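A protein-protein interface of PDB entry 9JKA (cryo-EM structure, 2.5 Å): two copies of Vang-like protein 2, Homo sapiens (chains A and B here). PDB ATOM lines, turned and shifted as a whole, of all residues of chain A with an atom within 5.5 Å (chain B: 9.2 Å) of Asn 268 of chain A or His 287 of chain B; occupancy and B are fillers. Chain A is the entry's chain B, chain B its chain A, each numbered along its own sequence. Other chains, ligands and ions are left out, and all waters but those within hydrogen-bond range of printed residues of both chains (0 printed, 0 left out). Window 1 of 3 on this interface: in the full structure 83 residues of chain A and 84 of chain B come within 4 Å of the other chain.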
ATOM      1  N   PRO A 250      16.361 -21.509  21.214  1.00  0.00           N
ATOM      2  CA  PRO A 250      15.326 -22.027  22.121  1.00  0.00           C
ATOM      3  C   PRO A 250      15.721 -23.373  22.710  1.00  0.00           C
ATOM      4  O   PRO A 250      16.011 -24.328  21.987  1.00  0.00           O
ATOM      5  CB  PRO A 250      14.092 -22.137  21.222  1.00  0.00           C
ATOM      6  CG  PRO A 250      14.633 -22.290  19.864  1.00  0.00           C
ATOM      7  CD  PRO A 250      15.913 -21.521  19.811  1.00  0.00           C
ATOM      8  N   PHE A 252      13.989 -24.576  25.892  1.00  0.00           N
ATOM      9  CA  PHE A 252      12.934 -25.104  26.737  1.00  0.00           C
ATOM     10  C   PHE A 252      11.578 -24.688  26.198  1.00  0.00           C
ATOM     11  O   PHE A 252      11.435 -23.637  25.573  1.00  0.00           O
ATOM     12  CB  PHE A 252      13.085 -24.610  28.175  1.00  0.00           C
ATOM     13  CG  PHE A 252      14.377 -25.006  28.808  1.00  0.00           C
ATOM     14  CD1 PHE A 252      14.555 -26.283  29.300  1.00  0.00           C
ATOM     15  CD2 PHE A 252      15.419 -24.103  28.898  1.00  0.00           C
ATOM     16  CE1 PHE A 252      15.747 -26.651  29.871  1.00  0.00           C
ATOM     17  CE2 PHE A 252      16.612 -24.465  29.467  1.00  0.00           C
ATOM     18  CZ  PHE A 252      16.776 -25.741  29.955  1.00  0.00           C
ATOM     19  N   THR A 253      10.583 -25.527  26.446  1.00  0.00           N
ATOM     20  CA  THR A 253       9.192 -25.212  26.178  1.00  0.00           C
ATOM     21  C   THR A 253       8.488 -24.983  27.506  1.00  0.00           C
ATOM     22  O   THR A 253       8.540 -25.832  28.401  1.00  0.00           O
ATOM     23  CB  THR A 253       8.502 -26.327  25.396  1.00  0.00           C
ATOM     24  OG1 THR A 253       9.188 -26.539  24.159  1.00  0.00           O
ATOM     25  CG2 THR A 253       7.069 -25.945  25.097  1.00  0.00           C
ATOM     26  N   LEU A 254       7.844 -23.833  27.625  1.00  0.00           N
ATOM     27  CA  LEU A 254       7.141 -23.414  28.823  1.00  0.00           C
ATOM     28  C   LEU A 254       5.649 -23.544  28.574  1.00  0.00           C
ATOM     29  O   LEU A 254       5.128 -22.953  27.625  1.00  0.00           O
ATOM     30  CB  LEU A 254       7.486 -21.970  29.164  1.00  0.00           C
ATOM     31  CG  LEU A 254       8.944 -21.654  29.448  1.00  0.00           C
ATOM     32  CD1 LEU A 254       9.104 -20.162  29.484  1.00  0.00           C
ATOM     33  CD2 LEU A 254       9.368 -22.262  30.755  1.00  0.00           C
ATOM     34  N   PHE A 266       1.940 -21.945  25.163  1.00  0.00           N
ATOM     35  CA  PHE A 266       3.260 -22.549  25.219  1.00  0.00           C
ATOM     36  C   PHE A 266       4.256 -21.613  24.553  1.00  0.00           C
ATOM     37  O   PHE A 266       3.924 -20.893  23.609  1.00  0.00           O
ATOM     38  CB  PHE A 266       3.388 -23.924  24.536  1.00  0.00           C
ATOM     39  CG  PHE A 266       2.628 -25.073  25.181  1.00  0.00           C
ATOM     40  CD1 PHE A 266       1.419 -24.921  25.834  1.00  0.00           C
ATOM     41  CD2 PHE A 266       3.254 -26.301  25.270  1.00  0.00           C
ATOM     42  CE1 PHE A 266       0.783 -25.988  26.413  1.00  0.00           C
ATOM     43  CE2 PHE A 266       2.647 -27.365  25.896  1.00  0.00           C
ATOM     44  CZ  PHE A 266       1.405 -27.210  26.460  1.00  0.00           C
ATOM     45  N   TYR A 267       5.484 -21.632  25.055  1.00  0.00           N
ATOM     46  CA  TYR A 267       6.520 -20.750  24.550  1.00  0.00           C
ATOM     47  C   TYR A 267       7.823 -21.519  24.430  1.00  0.00           C
ATOM     48  O   TYR A 267       8.035 -22.522  25.106  1.00  0.00           O
ATOM     49  CB  TYR A 267       6.726 -19.547  25.469  1.00  0.00           C
ATOM     50  CG  TYR A 267       5.491 -18.717  25.693  1.00  0.00           C
ATOM     51  CD1 TYR A 267       5.023 -17.858  24.714  1.00  0.00           C
ATOM     52  CD2 TYR A 267       4.800 -18.784  26.895  1.00  0.00           C
ATOM     53  CE1 TYR A 267       3.894 -17.103  24.919  1.00  0.00           C
ATOM     54  CE2 TYR A 267       3.674 -18.030  27.109  1.00  0.00           C
ATOM     55  CZ  TYR A 267       3.226 -17.193  26.119  1.00  0.00           C
ATOM     56  OH  TYR A 267       2.102 -16.442  26.336  1.00  0.00           O
ATOM     57  N   ASN A 268       8.703 -21.041  23.560  1.00  0.00           N
ATOM     58  CA  ASN A 268      10.085 -21.493  23.526  1.00  0.00           C
ATOM     59  C   ASN A 268      10.974 -20.420  24.127  1.00  0.00           C
ATOM     60  O   ASN A 268      10.913 -19.258  23.717  1.00  0.00           O
ATOM     61  CB  ASN A 268      10.556 -21.809  22.112  1.00  0.00           C
ATOM     62  CG  ASN A 268      10.126 -23.166  21.639  1.00  0.00           C
ATOM     63  OD1 ASN A 268      10.047 -24.113  22.416  1.00  0.00           O
ATOM     64  ND2 ASN A 268       9.922 -23.292  20.339  1.00  0.00           N
ATOM     65  N   VAL A 269      11.805 -20.817  25.079  1.00  0.00           N
ATOM     66  CA  VAL A 269      12.698 -19.901  25.764  1.00  0.00           C
ATOM     67  C   VAL A 269      14.095 -20.503  25.704  1.00  0.00           C
ATOM     68  O   VAL A 269      14.259 -21.711  25.516  1.00  0.00           O
ATOM     69  CB  VAL A 269      12.217 -19.647  27.217  1.00  0.00           C
ATOM     70  CG1 VAL A 269      12.485 -20.845  28.104  1.00  0.00           C
ATOM     71  CG2 VAL A 269      12.790 -18.361  27.795  1.00  0.00           C
ATOM     72  N   GLY A 270      15.106 -19.646  25.800  1.00  0.00           N
ATOM     73  CA  GLY A 270      16.486 -20.065  25.798  1.00  0.00           C
ATOM     74  C   GLY A 270      17.043 -20.213  27.195  1.00  0.00           C
ATOM     75  O   GLY A 270      16.311 -20.377  28.176  1.00  0.00           O
ATOM     76  N   TRP A 280       9.977 -12.447  31.288  1.00  0.00           N
ATOM     77  CA  TRP A 280       9.672 -12.747  29.893  1.00  0.00           C
ATOM     78  C   TRP A 280       8.238 -13.254  29.725  1.00  0.00           C
ATOM     79  O   TRP A 280       7.513 -12.833  28.811  1.00  0.00           O
ATOM     80  CB  TRP A 280      10.683 -13.783  29.418  1.00  0.00           C
ATOM     81  CG  TRP A 280      10.698 -14.077  27.991  1.00  0.00           C
ATOM     82  CD1 TRP A 280      11.208 -13.304  27.001  1.00  0.00           C
ATOM     83  CD2 TRP A 280      10.168 -15.239  27.365  1.00  0.00           C
ATOM     84  NE1 TRP A 280      11.041 -13.919  25.791  1.00  0.00           N
ATOM     85  CE2 TRP A 280      10.398 -15.110  25.989  1.00  0.00           C
ATOM     86  CE3 TRP A 280       9.517 -16.378  27.838  1.00  0.00           C
ATOM     87  CZ2 TRP A 280      10.008 -16.075  25.080  1.00  0.00           C
ATOM     88  CZ3 TRP A 280       9.130 -17.330  26.939  1.00  0.00           C
ATOM     89  CH2 TRP A 280       9.372 -17.175  25.573  1.00  0.00           C
ATOM     90  N   VAL A 500      13.310 -28.978  25.207  1.00  0.00           N
ATOM     91  CA  VAL A 500      13.090 -29.207  23.781  1.00  0.00           C
ATOM     92  C   VAL A 500      13.898 -30.431  23.376  1.00  0.00           C
ATOM     93  O   VAL A 500      15.117 -30.466  23.608  1.00  0.00           O
ATOM     94  CB  VAL A 500      13.483 -27.971  22.955  1.00  0.00           C
ATOM     95  CG1 VAL A 500      13.389 -28.264  21.470  1.00  0.00           C
ATOM     96  CG2 VAL A 500      12.593 -26.802  23.307  1.00  0.00           C
ATOM     97  N   ARG B 265       0.129 -23.949  10.411  1.00  0.00           N
ATOM     98  CA  ARG B 265       0.628 -22.711  10.992  1.00  0.00           C
ATOM     99  C   ARG B 265       1.541 -22.019   9.998  1.00  0.00           C
ATOM    100  O   ARG B 265       2.165 -22.664   9.152  1.00  0.00           O
ATOM    101  CB  ARG B 265       1.400 -22.927  12.298  1.00  0.00           C
ATOM    102  CG  ARG B 265       0.608 -23.505  13.448  1.00  0.00           C
ATOM    103  CD  ARG B 265      -0.475 -22.621  13.983  1.00  0.00           C
ATOM    104  NE  ARG B 265      -1.033 -23.218  15.189  1.00  0.00           N
ATOM    105  CZ  ARG B 265      -2.016 -24.113  15.198  1.00  0.00           C
ATOM    106  NH1 ARG B 265      -2.560 -24.520  14.061  1.00  0.00           N
ATOM    107  NH2 ARG B 265      -2.455 -24.603  16.348  1.00  0.00           N
ATOM    108  N   TYR B 267       4.834 -19.233   9.584  1.00  0.00           N
ATOM    109  CA  TYR B 267       5.965 -18.712  10.329  1.00  0.00           C
ATOM    110  C   TYR B 267       6.764 -17.774   9.442  1.00  0.00           C
ATOM    111  O   TYR B 267       6.722 -17.867   8.218  1.00  0.00           O
ATOM    112  CB  TYR B 267       6.872 -19.836  10.825  1.00  0.00           C
ATOM    113  CG  TYR B 267       6.185 -20.853  11.695  1.00  0.00           C
ATOM    114  CD1 TYR B 267       5.865 -20.566  13.009  1.00  0.00           C
ATOM    115  CD2 TYR B 267       5.870 -22.111  11.201  1.00  0.00           C
ATOM    116  CE1 TYR B 267       5.235 -21.493  13.802  1.00  0.00           C
ATOM    117  CE2 TYR B 267       5.243 -23.045  11.986  1.00  0.00           C
ATOM    118  CZ  TYR B 267       4.930 -22.731  13.284  1.00  0.00           C
ATOM    119  OH  TYR B 267       4.306 -23.667  14.067  1.00  0.00           O
ATOM    120  N   VAL B 279      14.753 -28.142  11.515  1.00  0.00           N
ATOM    121  CA  VAL B 279      14.881 -28.253  12.970  1.00  0.00           C
ATOM    122  C   VAL B 279      14.112 -27.132  13.668  1.00  0.00           C
ATOM    123  O   VAL B 279      13.475 -27.345  14.709  1.00  0.00           O
ATOM    124  CB  VAL B 279      16.368 -28.267  13.362  1.00  0.00           C
ATOM    125  CG1 VAL B 279      16.548 -28.203  14.859  1.00  0.00           C
ATOM    126  CG2 VAL B 279      16.997 -29.519  12.851  1.00  0.00           C
ATOM    127  N   TRP B 280      14.121 -25.937  13.075  1.00  0.00           N
ATOM    128  CA  TRP B 280      13.367 -24.801  13.595  1.00  0.00           C
ATOM    129  C   TRP B 280      11.861 -25.076  13.591  1.00  0.00           C
ATOM    130  O   TRP B 280      11.156 -24.786  14.569  1.00  0.00           O
ATOM    131  CB  TRP B 280      13.708 -23.594  12.730  1.00  0.00           C
ATOM    132  CG  TRP B 280      13.226 -22.299  13.194  1.00  0.00           C
ATOM    133  CD1 TRP B 280      13.725 -21.559  14.213  1.00  0.00           C
ATOM    134  CD2 TRP B 280      12.128 -21.570  12.662  1.00  0.00           C
ATOM    135  NE1 TRP B 280      13.013 -20.398  14.345  1.00  0.00           N
ATOM    136  CE2 TRP B 280      12.020 -20.385  13.402  1.00  0.00           C
ATOM    137  CE3 TRP B 280      11.222 -21.807  11.629  1.00  0.00           C
ATOM    138  CZ2 TRP B 280      11.048 -19.437  13.144  1.00  0.00           C
ATOM    139  CZ3 TRP B 280      10.261 -20.870  11.375  1.00  0.00           C
ATOM    140  CH2 TRP B 280      10.178 -19.698  12.130  1.00  0.00           C
ATOM    141  N   ILE B 281      11.365 -25.680  12.510  1.00  0.00           N
ATOM    142  CA  ILE B 281       9.956 -26.044  12.403  1.00  0.00           C
ATOM    143  C   ILE B 281       9.612 -27.158  13.379  1.00  0.00           C
ATOM    144  O   ILE B 281       8.526 -27.168  13.959  1.00  0.00           O
ATOM    145  CB  ILE B 281       9.624 -26.419  10.945  1.00  0.00           C
ATOM    146  CG1 ILE B 281       9.653 -25.179  10.070  1.00  0.00           C
ATOM    147  CG2 ILE B 281       8.264 -27.075  10.795  1.00  0.00           C
ATOM    148  CD1 ILE B 281       9.647 -25.512   8.635  1.00  0.00           C
ATOM    149  N   LEU B 282      10.536 -28.091  13.613  1.00  0.00           N
ATOM    150  CA  LEU B 282      10.253 -29.144  14.583  1.00  0.00           C
ATOM    151  C   LEU B 282      10.245 -28.617  16.009  1.00  0.00           C
ATOM    152  O   LEU B 282       9.543 -29.161  16.866  1.00  0.00           O
ATOM    153  CB  LEU B 282      11.257 -30.281  14.451  1.00  0.00           C
ATOM    154  CG  LEU B 282      11.147 -31.059  13.148  1.00  0.00           C
ATOM    155  CD1 LEU B 282      12.176 -32.161  13.108  1.00  0.00           C
ATOM    156  CD2 LEU B 282       9.749 -31.578  12.956  1.00  0.00           C
ATOM    157  N   GLU B 283      11.014 -27.565  16.280  1.00  0.00           N
ATOM    158  CA  GLU B 283      10.920 -26.899  17.573  1.00  0.00           C
ATOM    159  C   GLU B 283       9.600 -26.151  17.713  1.00  0.00           C
ATOM    160  O   GLU B 283       9.031 -26.088  18.808  1.00  0.00           O
ATOM    161  CB  GLU B 283      12.097 -25.952  17.750  1.00  0.00           C
ATOM    162  CG  GLU B 283      13.400 -26.675  17.930  1.00  0.00           C
ATOM    163  CD  GLU B 283      14.586 -25.751  17.909  1.00  0.00           C
ATOM    164  OE1 GLU B 283      14.416 -24.566  17.561  1.00  0.00           O
ATOM    165  OE2 GLU B 283      15.693 -26.212  18.245  1.00  0.00           O
ATOM    166  N   LYS B 284       9.104 -25.572  16.620  1.00  0.00           N
ATOM    167  CA  LYS B 284       7.788 -24.939  16.672  1.00  0.00           C
ATOM    168  C   LYS B 284       6.656 -25.959  16.728  1.00  0.00           C
ATOM    169  O   LYS B 284       5.573 -25.649  17.236  1.00  0.00           O
ATOM    170  CB  LYS B 284       7.589 -24.023  15.468  1.00  0.00           C
ATOM    171  CG  LYS B 284       8.511 -22.837  15.428  1.00  0.00           C
ATOM    172  CD  LYS B 284       8.195 -21.899  16.565  1.00  0.00           C
ATOM    173  CE  LYS B 284       9.058 -20.666  16.502  1.00  0.00           C
ATOM    174  NZ  LYS B 284       8.668 -19.833  15.339  1.00  0.00           N
ATOM    175  N   TYR B 285       6.881 -27.165  16.201  1.00  0.00           N
ATOM    176  CA  TYR B 285       5.803 -28.133  16.027  1.00  0.00           C
ATOM    177  C   TYR B 285       5.331 -28.698  17.356  1.00  0.00           C
ATOM    178  O   TYR B 285       4.129 -28.913  17.550  1.00  0.00           O
ATOM    179  CB  TYR B 285       6.248 -29.270  15.099  1.00  0.00           C
ATOM    180  CG  TYR B 285       5.249 -30.403  15.071  1.00  0.00           C
ATOM    181  CD1 TYR B 285       4.037 -30.261  14.431  1.00  0.00           C
ATOM    182  CD2 TYR B 285       5.510 -31.605  15.711  1.00  0.00           C
ATOM    183  CE1 TYR B 285       3.120 -31.279  14.426  1.00  0.00           C
ATOM    184  CE2 TYR B 285       4.585 -32.625  15.718  1.00  0.00           C
ATOM    185  CZ  TYR B 285       3.395 -32.450  15.069  1.00  0.00           C
ATOM    186  OH  TYR B 285       2.447 -33.434  15.052  1.00  0.00           O
ATOM    187  N   TYR B 286       6.254 -28.952  18.277  1.00  0.00           N
ATOM    188  CA  TYR B 286       5.882 -29.622  19.513  1.00  0.00           C
ATOM    189  C   TYR B 286       5.089 -28.742  20.459  1.00  0.00           C
ATOM    190  O   TYR B 286       4.486 -29.272  21.394  1.00  0.00           O
ATOM    191  CB  TYR B 286       7.132 -30.175  20.189  1.00  0.00           C
ATOM    192  CG  TYR B 286       7.590 -31.465  19.557  1.00  0.00           C
ATOM    193  CD1 TYR B 286       6.706 -32.255  18.851  1.00  0.00           C
ATOM    194  CD2 TYR B 286       8.900 -31.880  19.634  1.00  0.00           C
ATOM    195  CE1 TYR B 286       7.102 -33.426  18.260  1.00  0.00           C
ATOM    196  CE2 TYR B 286       9.302 -33.061  19.045  1.00  0.00           C
ATOM    197  CZ  TYR B 286       8.400 -33.823  18.356  1.00  0.00           C
ATOM    198  OH  TYR B 286       8.795 -34.992  17.764  1.00  0.00           O
ATOM    199  N   HIS B 287       5.025 -27.435  20.230  1.00  0.00           N
ATOM    200  CA  HIS B 287       4.168 -26.598  21.042  1.00  0.00           C
ATOM    201  C   HIS B 287       3.126 -25.825  20.247  1.00  0.00           C
ATOM    202  O   HIS B 287       2.254 -25.203  20.860  1.00  0.00           O
ATOM    203  CB  HIS B 287       5.004 -25.618  21.877  1.00  0.00           C
ATOM    204  CG  HIS B 287       5.575 -24.479  21.097  1.00  0.00           C
ATOM    205  ND1 HIS B 287       4.911 -23.283  20.940  1.00  0.00           N
ATOM    206  CD2 HIS B 287       6.746 -24.349  20.435  1.00  0.00           C
ATOM    207  CE1 HIS B 287       5.646 -22.465  20.212  1.00  0.00           C
ATOM    208  NE2 HIS B 287       6.765 -23.088  19.892  1.00  0.00           N
ATOM    209  N   ASP B 288       3.173 -25.842  18.915  1.00  0.00           N
ATOM    210  CA  ASP B 288       2.196 -25.099  18.125  1.00  0.00           C
ATOM    211  C   ASP B 288       1.060 -25.955  17.582  1.00  0.00           C
ATOM    212  O   ASP B 288      -0.099 -25.548  17.672  1.00  0.00           O
ATOM    213  CB  ASP B 288       2.880 -24.369  16.967  1.00  0.00           C
ATOM    214  CG  ASP B 288       3.544 -23.083  17.400  1.00  0.00           C
ATOM    215  OD1 ASP B 288       3.062 -22.463  18.367  1.00  0.00           O
ATOM    216  OD2 ASP B 288       4.536 -22.679  16.764  1.00  0.00           O
ATOM    217  N   PHE B 289       1.352 -27.117  17.004  1.00  0.00           N
ATOM    218  CA  PHE B 289       0.249 -27.881  16.440  1.00  0.00           C
ATOM    219  C   PHE B 289      -0.393 -28.691  17.552  1.00  0.00           C
ATOM    220  O   PHE B 289       0.252 -28.967  18.558  1.00  0.00           O
ATOM    221  CB  PHE B 289       0.678 -28.867  15.348  1.00  0.00           C
ATOM    222  CG  PHE B 289       1.207 -28.271  14.058  1.00  0.00           C
ATOM    223  CD1 PHE B 289       1.677 -26.981  13.934  1.00  0.00           C
ATOM    224  CD2 PHE B 289       1.087 -29.018  12.906  1.00  0.00           C
ATOM    225  CE1 PHE B 289       2.142 -26.521  12.729  1.00  0.00           C
ATOM    226  CE2 PHE B 289       1.524 -28.543  11.705  1.00  0.00           C
ATOM    227  CZ  PHE B 289       2.036 -27.290  11.618  1.00  0.00           C
ATOM    228  N   PRO B 290      -1.653 -29.093  17.401  1.00  0.00           N
ATOM    229  CA  PRO B 290      -2.200 -30.122  18.290  1.00  0.00           C
ATOM    230  C   PRO B 290      -1.490 -31.451  18.089  1.00  0.00           C
ATOM    231  O   PRO B 290      -0.856 -31.699  17.062  1.00  0.00           O
ATOM    232  CB  PRO B 290      -3.671 -30.210  17.875  1.00  0.00           C
ATOM    233  CG  PRO B 290      -3.966 -28.889  17.290  1.00  0.00           C
ATOM    234  CD  PRO B 290      -2.711 -28.470  16.587  1.00  0.00           C
ATOM    235  N   VAL B 291      -1.587 -32.304  19.111  1.00  0.00           N
ATOM    236  CA  VAL B 291      -0.925 -33.601  19.075  1.00  0.00           C
ATOM    237  C   VAL B 291      -1.572 -34.472  18.002  1.00  0.00           C
ATOM    238  O   VAL B 291      -2.766 -34.344  17.698  1.00  0.00           O
ATOM    239  CB  VAL B 291      -0.968 -34.254  20.474  1.00  0.00           C
ATOM    240  CG1 VAL B 291      -2.388 -34.626  20.879  1.00  0.00           C
ATOM    241  CG2 VAL B 291      -0.020 -35.441  20.580  1.00  0.00           C
ATOM    242  N   GLY B 451      -4.454 -30.288  22.575  1.00  0.00           N
ATOM    243  CA  GLY B 451      -3.202 -29.782  23.080  1.00  0.00           C
ATOM    244  C   GLY B 451      -2.015 -30.283  22.287  1.00  0.00           C
ATOM    245  O   GLY B 451      -2.112 -31.246  21.525  1.00  0.00           O
ATOM    246  N   PRO B 452      -0.872 -29.639  22.444  1.00  0.00           N
ATOM    247  CA  PRO B 452       0.289 -29.957  21.613  1.00  0.00           C
ATOM    248  C   PRO B 452       1.027 -31.208  22.071  1.00  0.00           C
ATOM    249  O   PRO B 452       0.702 -31.826  23.077  1.00  0.00           O
ATOM    250  CB  PRO B 452       1.156 -28.710  21.747  1.00  0.00           C
ATOM    251  CG  PRO B 452       0.781 -28.134  23.004  1.00  0.00           C
ATOM    252  CD  PRO B 452      -0.658 -28.414  23.223  1.00  0.00           C
ATOM    253  N   THR B 453       2.046 -31.565  21.290  1.00  0.00           N
ATOM    254  CA  THR B 453       2.704 -32.857  21.431  1.00  0.00           C
ATOM    255  C   THR B 453       3.608 -32.896  22.655  1.00  0.00           C
ATOM    256  O   THR B 453       3.725 -33.935  23.314  1.00  0.00           O
ATOM    257  CB  THR B 453       3.490 -33.161  20.154  1.00  0.00           C
ATOM    258  OG1 THR B 453       2.615 -33.053  19.028  1.00  0.00           O
ATOM    259  CG2 THR B 453       4.069 -34.561  20.174  1.00  0.00           C
ATOM    260  N   ILE B 454       4.218 -31.763  23.013  1.00  0.00           N
ATOM    261  CA  ILE B 454       5.151 -31.754  24.133  1.00  0.00           C
ATOM    262  C   ILE B 454       4.408 -31.781  25.464  1.00  0.00           C
ATOM    263  O   ILE B 454       5.010 -32.033  26.508  1.00  0.00           O
ATOM    264  CB  ILE B 454       6.096 -30.537  24.020  1.00  0.00           C
ATOM    265  CG1 ILE B 454       7.401 -30.788  24.775  1.00  0.00           C
ATOM    266  CG2 ILE B 454       5.428 -29.291  24.559  1.00  0.00           C
ATOM    267  CD1 ILE B 454       8.512 -29.877  24.387  1.00  0.00           C
ATOM    268  N   GLN B 455       3.087 -31.595  25.440  1.00  0.00           N
ATOM    269  CA  GLN B 455       2.280 -31.689  26.651  1.00  0.00           C
ATOM    270  C   GLN B 455       2.212 -33.126  27.166  1.00  0.00           C
ATOM    271  O   GLN B 455       1.903 -33.358  28.339  1.00  0.00           O
ATOM    272  CB  GLN B 455       0.884 -31.148  26.349  1.00  0.00           C
ATOM    273  CG  GLN B 455      -0.005 -30.860  27.531  1.00  0.00           C
ATOM    274  CD  GLN B 455      -1.332 -30.302  27.092  1.00  0.00           C
ATOM    275  OE1 GLN B 455      -1.630 -30.264  25.908  1.00  0.00           O
ATOM    276  NE2 GLN B 455      -2.121 -29.829  28.038  1.00  0.00           N
ATOM    277  N   TRP B 461       6.553 -38.340  21.680  1.00  0.00           N
ATOM    278  CA  TRP B 461       7.246 -37.293  20.938  1.00  0.00           C
ATOM    279  C   TRP B 461       7.894 -37.866  19.685  1.00  0.00           C
ATOM    280  O   TRP B 461       7.611 -37.415  18.568  1.00  0.00           O
ATOM    281  CB  TRP B 461       8.298 -36.623  21.825  1.00  0.00           C
ATOM    282  CG  TRP B 461       7.757 -35.905  23.033  1.00  0.00           C
ATOM    283  CD1 TRP B 461       6.448 -35.702  23.358  1.00  0.00           C
ATOM    284  CD2 TRP B 461       8.525 -35.289  24.072  1.00  0.00           C
ATOM    285  NE1 TRP B 461       6.354 -35.011  24.537  1.00  0.00           N
ATOM    286  CE2 TRP B 461       7.616 -34.742  24.994  1.00  0.00           C
ATOM    287  CE3 TRP B 461       9.894 -35.151  24.312  1.00  0.00           C
ATOM    288  CZ2 TRP B 461       8.030 -34.069  26.138  1.00  0.00           C
ATOM    289  CZ3 TRP B 461      10.303 -34.481  25.446  1.00  0.00           C
ATOM    290  CH2 TRP B 461       9.375 -33.948  26.345  1.00  0.00           C
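The side-chain amide nitrogen (ND2) of Asn 268 of chain A lies within hydrogen-bond range of the backbone carbonyl oxygen (O) of Glu 283 of chain B, at 3.3 Å.
NE2 of His 287 of chain B sits at hydrogen-bond distance from ND2 of Asn 268 of chain A (3.2 Å).
Of the 11 printed residues of chain A, 5 touch a printed residue of chain B.
Hydrophobic or aromatic side chains of chain A that line the printed part of chain B: Pro 250, Phe 266 and Val 500.
Hydrophobic or aromatic side chains of chain B within 4 Å of the printed part of chain A: His 287, Pro 452 and Ile 454.
Among the printed residues, no Asp or Glu carboxylate lies within 4 Å of a Lys or Arg side-chain nitrogen of the other chain.
Positions printed for both chains: 267 and 280.
Printed residues of chain B within 4 Å of Thr 253 of chain A: His 287 (3.8 Å) and Ile 454 (3.4 Å).
Of the printed residues of chain B, Asn 268 of chain A touches Glu 283 and His 287.
Val 269 of chain A touches none of the printed residues of chain B.
Of the printed residues of chain B, Val 500 of chain A touches Glu 283 (3.9 Å).
Printed residues of chain A within 4 Å of Glu 283 of chain B: Pro 250, Asn 268 and Val 500.
Of the printed residues of chain A, Gln 455 of chain B touches Phe 266 (3.97 Å).
Glu 283 of chain B touches Pro 250 of chain A.
CB of His 287 of chain B touches CG2 of Thr 253 of chain A, at 3.8 Å.
OG1 of Thr 253 of chain A touches CD1 of Ile 454 of chain B, 3.4 Å away.
Phe 266 of chain A touches His 287 of chain B (CB to CB, 3.5 Å).
Pro 452 of chain B touches Phe 266 of chain A (CG to CE2, 3.5 Å).
Phe 266 of chain A touches Ile 454 of chain B (CE2 to CG2, 3.6 Å).
Phe 266 of chain A touches Gln 455 of chain B (CZ to CB, 3.97 Å).
Glu 283 of chain B touches Val 500 of chain A (CG to CG1, 3.9 Å).
The backbone NH of Ile 454 of chain B lies within hydrogen-bond range of the backbone carbonyl oxygen of Tyr 286 of chain B (3.0 Å).
ND1 of His 287 of chain B sits close to OD1 of Asp 288 of chain B (3.3 Å).
The backbone carbonyl oxygen (O) of Phe 252 of chain A sits close to the side-chain amide oxygen (OD1) of Asn 268 of chain A (3.5 Å).
The side-chain hydroxyl (OG1) of Thr 253 of chain A sits at hydrogen-bond distance from the side-chain amide oxygen (OD1) of Asn 268 of chain A (3.1 Å).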
